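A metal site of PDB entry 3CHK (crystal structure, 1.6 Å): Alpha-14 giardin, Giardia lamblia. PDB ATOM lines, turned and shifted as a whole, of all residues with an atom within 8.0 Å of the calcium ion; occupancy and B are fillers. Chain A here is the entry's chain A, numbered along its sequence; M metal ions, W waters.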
ATOM      1  N   ASN A 252      -2.601  -2.721  10.352  1.00  0.00           N
ATOM      2  CA  ASN A 252      -2.327  -2.124  11.677  1.00  0.00           C
ATOM      3  C   ASN A 252      -0.912  -1.568  11.752  1.00  0.00           C
ATOM      4  O   ASN A 252      -0.664  -0.480  12.255  1.00  0.00           O
ATOM      5  CB  ASN A 252      -2.565  -3.150  12.778  1.00  0.00           C
ATOM      6  CG  ASN A 252      -2.332  -2.554  14.153  1.00  0.00           C
ATOM      7  OD1 ASN A 252      -1.298  -2.756  14.736  1.00  0.00           O
ATOM      8  ND2 ASN A 252      -3.317  -1.810  14.644  1.00  0.00           N
ATOM      9  N   VAL A 253       0.042  -2.335  11.223  1.00  0.00           N
ATOM     10  CA  VAL A 253       1.436  -1.910  11.222  1.00  0.00           C
ATOM     11  C   VAL A 253       1.599  -0.621  10.400  1.00  0.00           C
ATOM     12  O   VAL A 253       2.317   0.291  10.833  1.00  0.00           O
ATOM     13  CB  VAL A 253       2.387  -3.023  10.799  1.00  0.00           C
ATOM     14  CG1 VAL A 253       3.823  -2.492  10.702  1.00  0.00           C
ATOM     15  CG2 VAL A 253       2.315  -4.175  11.828  1.00  0.00           C
ATOM     16  N   ALA A 254       0.906  -0.534   9.267  1.00  0.00           N
ATOM     17  CA  ALA A 254       1.005   0.657   8.392  1.00  0.00           C
ATOM     18  C   ALA A 254       0.466   1.899   9.078  1.00  0.00           C
ATOM     19  O   ALA A 254       0.946   3.004   8.804  1.00  0.00           O
ATOM     20  CB  ALA A 254       0.275   0.415   7.066  1.00  0.00           C
ATOM     21  N   PHE A 255      -0.534   1.730   9.950  1.00  0.00           N
ATOM     22  CA  PHE A 255      -1.141   2.868  10.657  1.00  0.00           C
ATOM     23  C   PHE A 255      -0.280   3.270  11.844  1.00  0.00           C
ATOM     24  O   PHE A 255      -0.478   4.363  12.378  1.00  0.00           O
ATOM     25  CB  PHE A 255      -2.500   2.503  11.256  1.00  0.00           C
ATOM     26  CG  PHE A 255      -3.633   2.370  10.244  1.00  0.00           C
ATOM     27  CD1 PHE A 255      -3.824   3.320   9.241  1.00  0.00           C
ATOM     28  CD2 PHE A 255      -4.570   1.333  10.374  1.00  0.00           C
ATOM     29  CE1 PHE A 255      -4.892   3.187   8.339  1.00  0.00           C
ATOM     30  CE2 PHE A 255      -5.661   1.231   9.492  1.00  0.00           C
ATOM     31  CZ  PHE A 255      -5.805   2.166   8.477  1.00  0.00           C
ATOM     32  N   ALA A 256       0.593   2.382  12.314  1.00  0.00           N
ATOM     33  CA  ALA A 256       1.296   2.582  13.588  1.00  0.00           C
ATOM     34  C   ALA A 256       2.217   3.780  13.587  1.00  0.00           C
ATOM     35  O   ALA A 256       2.914   4.042  12.604  1.00  0.00           O
ATOM     36  CB  ALA A 256       2.069   1.310  13.973  1.00  0.00           C
ATOM     37  N   GLY A 257       2.242   4.504  14.703  1.00  0.00           N
ATOM     38  CA  GLY A 257       3.150   5.635  14.860  1.00  0.00           C
ATOM     39  C   GLY A 257       2.534   6.885  14.305  1.00  0.00           C
ATOM     40  O   GLY A 257       1.369   6.894  13.876  1.00  0.00           O
ATOM     41  N   SER A 258       3.302   7.969  14.320  1.00  0.00           N
ATOM     42  CA  SER A 258       2.779   9.232  13.810  1.00  0.00           C
ATOM     43  C   SER A 258       2.572   9.112  12.321  1.00  0.00           C
ATOM     44  O   SER A 258       3.390   8.516  11.606  1.00  0.00           O
ATOM     45  CB  SER A 258       3.712  10.389  14.161  1.00  0.00           C
ATOM     46  OG  SER A 258       3.501  10.742  15.511  1.00  0.00           O
ATOM     47  N   GLY A 259       1.445   9.648  11.854  1.00  0.00           N
ATOM     48  CA  GLY A 259       1.126   9.565  10.445  1.00  0.00           C
ATOM     49  C   GLY A 259       0.805   8.128  10.063  1.00  0.00           C
ATOM     50  O   GLY A 259       0.313   7.351  10.870  1.00  0.00           O
ATOM     51  N   SER A 260       1.080   7.785   8.815  1.00  0.00           N
ATOM     52  CA  SER A 260       0.931   6.391   8.394  1.00  0.00           C
ATOM     53  C   SER A 260       1.601   6.168   7.061  1.00  0.00           C
ATOM     54  O   SER A 260       1.984   7.119   6.373  1.00  0.00           O
ATOM     55  CB  SER A 260      -0.523   6.000   8.339  1.00  0.00           C
ATOM     56  OG  SER A 260      -1.196   6.748   7.356  1.00  0.00           O
ATOM     57  N   ASP A 261       1.735   4.892   6.700  1.00  0.00           N
ATOM     58  CA  ASP A 261       2.568   4.502   5.578  1.00  0.00           C
ATOM     59  C   ASP A 261       1.583   4.230   4.465  1.00  0.00           C
ATOM     60  O   ASP A 261       1.018   3.119   4.354  1.00  0.00           O
ATOM     61  CB  ASP A 261       3.413   3.279   5.987  1.00  0.00           C
ATOM     62  CG  ASP A 261       4.382   2.837   4.901  1.00  0.00           C
ATOM     63  OD1 ASP A 261       4.263   3.268   3.729  1.00  0.00           O
ATOM     64  OD2 ASP A 261       5.256   2.007   5.204  1.00  0.00           O
ATOM     65  N   ARG A 294     -10.380   3.359  13.159  1.00  0.00           N
ATOM     66  CA  ARG A 294      -8.980   3.669  13.007  1.00  0.00           C
ATOM     67  C   ARG A 294      -8.755   4.473  11.723  1.00  0.00           C
ATOM     68  O   ARG A 294      -8.031   5.432  11.739  1.00  0.00           O
ATOM     69  CB  ARG A 294      -8.076   2.429  13.040  1.00  0.00           C
ATOM     70  CG  ARG A 294      -6.604   2.728  12.986  1.00  0.00           C
ATOM     71  CD  ARG A 294      -6.090   3.600  14.197  1.00  0.00           C
ATOM     72  NE  ARG A 294      -4.644   3.787  14.173  1.00  0.00           N
ATOM     73  CZ  ARG A 294      -3.770   2.920  14.728  1.00  0.00           C
ATOM     74  NH1 ARG A 294      -4.214   1.791  15.269  1.00  0.00           N
ATOM     75  NH2 ARG A 294      -2.465   3.168  14.690  1.00  0.00           N
ATOM     76  N   THR A 297      -9.418   8.253  12.016  1.00  0.00           N
ATOM     77  CA  THR A 297      -8.399   9.078  12.685  1.00  0.00           C
ATOM     78  C   THR A 297      -7.057   9.101  11.990  1.00  0.00           C
ATOM     79  O   THR A 297      -6.217   9.949  12.306  1.00  0.00           O
ATOM     80  CB  THR A 297      -8.274   8.760  14.201  1.00  0.00           C
ATOM     81  OG1 THR A 297      -7.867   7.387  14.379  1.00  0.00           O
ATOM     82  CG2 THR A 297      -9.607   8.988  14.909  1.00  0.00           C
ATOM     83  N   GLU A 298      -6.863   8.211  11.012  1.00  0.00           N
ATOM     84  CA  GLU A 298      -5.626   8.100  10.278  1.00  0.00           C
ATOM     85  C   GLU A 298      -5.711   8.783   8.907  1.00  0.00           C
ATOM     86  O   GLU A 298      -4.773   9.425   8.505  1.00  0.00           O
ATOM     87  CB  GLU A 298      -5.249   6.625  10.046  1.00  0.00           C
ATOM     88  CG  GLU A 298      -4.905   5.868  11.323  1.00  0.00           C
ATOM     89  CD  GLU A 298      -3.543   6.146  11.855  1.00  0.00           C
ATOM     90  OE1 GLU A 298      -2.651   6.552  11.079  1.00  0.00           O
ATOM     91  OE2 GLU A 298      -3.321   5.919  13.065  1.00  0.00           O
ATOM     92  N   LEU A 299      -6.817   8.551   8.206  1.00  0.00           N
ATOM     93  CA  LEU A 299      -6.894   8.982   6.808  1.00  0.00           C
ATOM     94  C   LEU A 299      -7.982  10.001   6.607  1.00  0.00           C
ATOM     95  O   LEU A 299      -8.960  10.075   7.365  1.00  0.00           O
ATOM     96  CB  LEU A 299      -7.134   7.778   5.886  1.00  0.00           C
ATOM     97  CG  LEU A 299      -6.102   6.652   6.022  1.00  0.00           C
ATOM     98  CD1 LEU A 299      -6.515   5.498   5.038  1.00  0.00           C
ATOM     99  CD2 LEU A 299      -4.654   7.085   5.888  1.00  0.00           C
HETATM  100 CA    CA M   1      -0.758   6.598  12.871  1.00  0.00          CA
HETATM  101  O   HOH W   1      -0.975   5.901  15.167  1.00  0.00           O
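O of Phe 255 sits close to NH2 of Arg 294 (3.3 Å).
The side-chain carboxylate (OE2) of Glu 298 sits close to the guanidinium group (NE) of Arg 294, 2.7 Å away.
Within 4 Å of the calcium ion: Phe 255, Gly 257, Gly 259 and Glu 298.
The nearest printed residue that does not touch the calcium ion is Ala 256 (4.2 Å).
The calcium ion is bound by O of Phe 255 (2.3 Å), O of Gly 257 (2.4 Å), O of Gly 259 (2.4 Å), water W1 (2.4 Å), OE1 of Glu 298 (2.6 Å) and OE2 of Glu 298 (2.7 Å).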
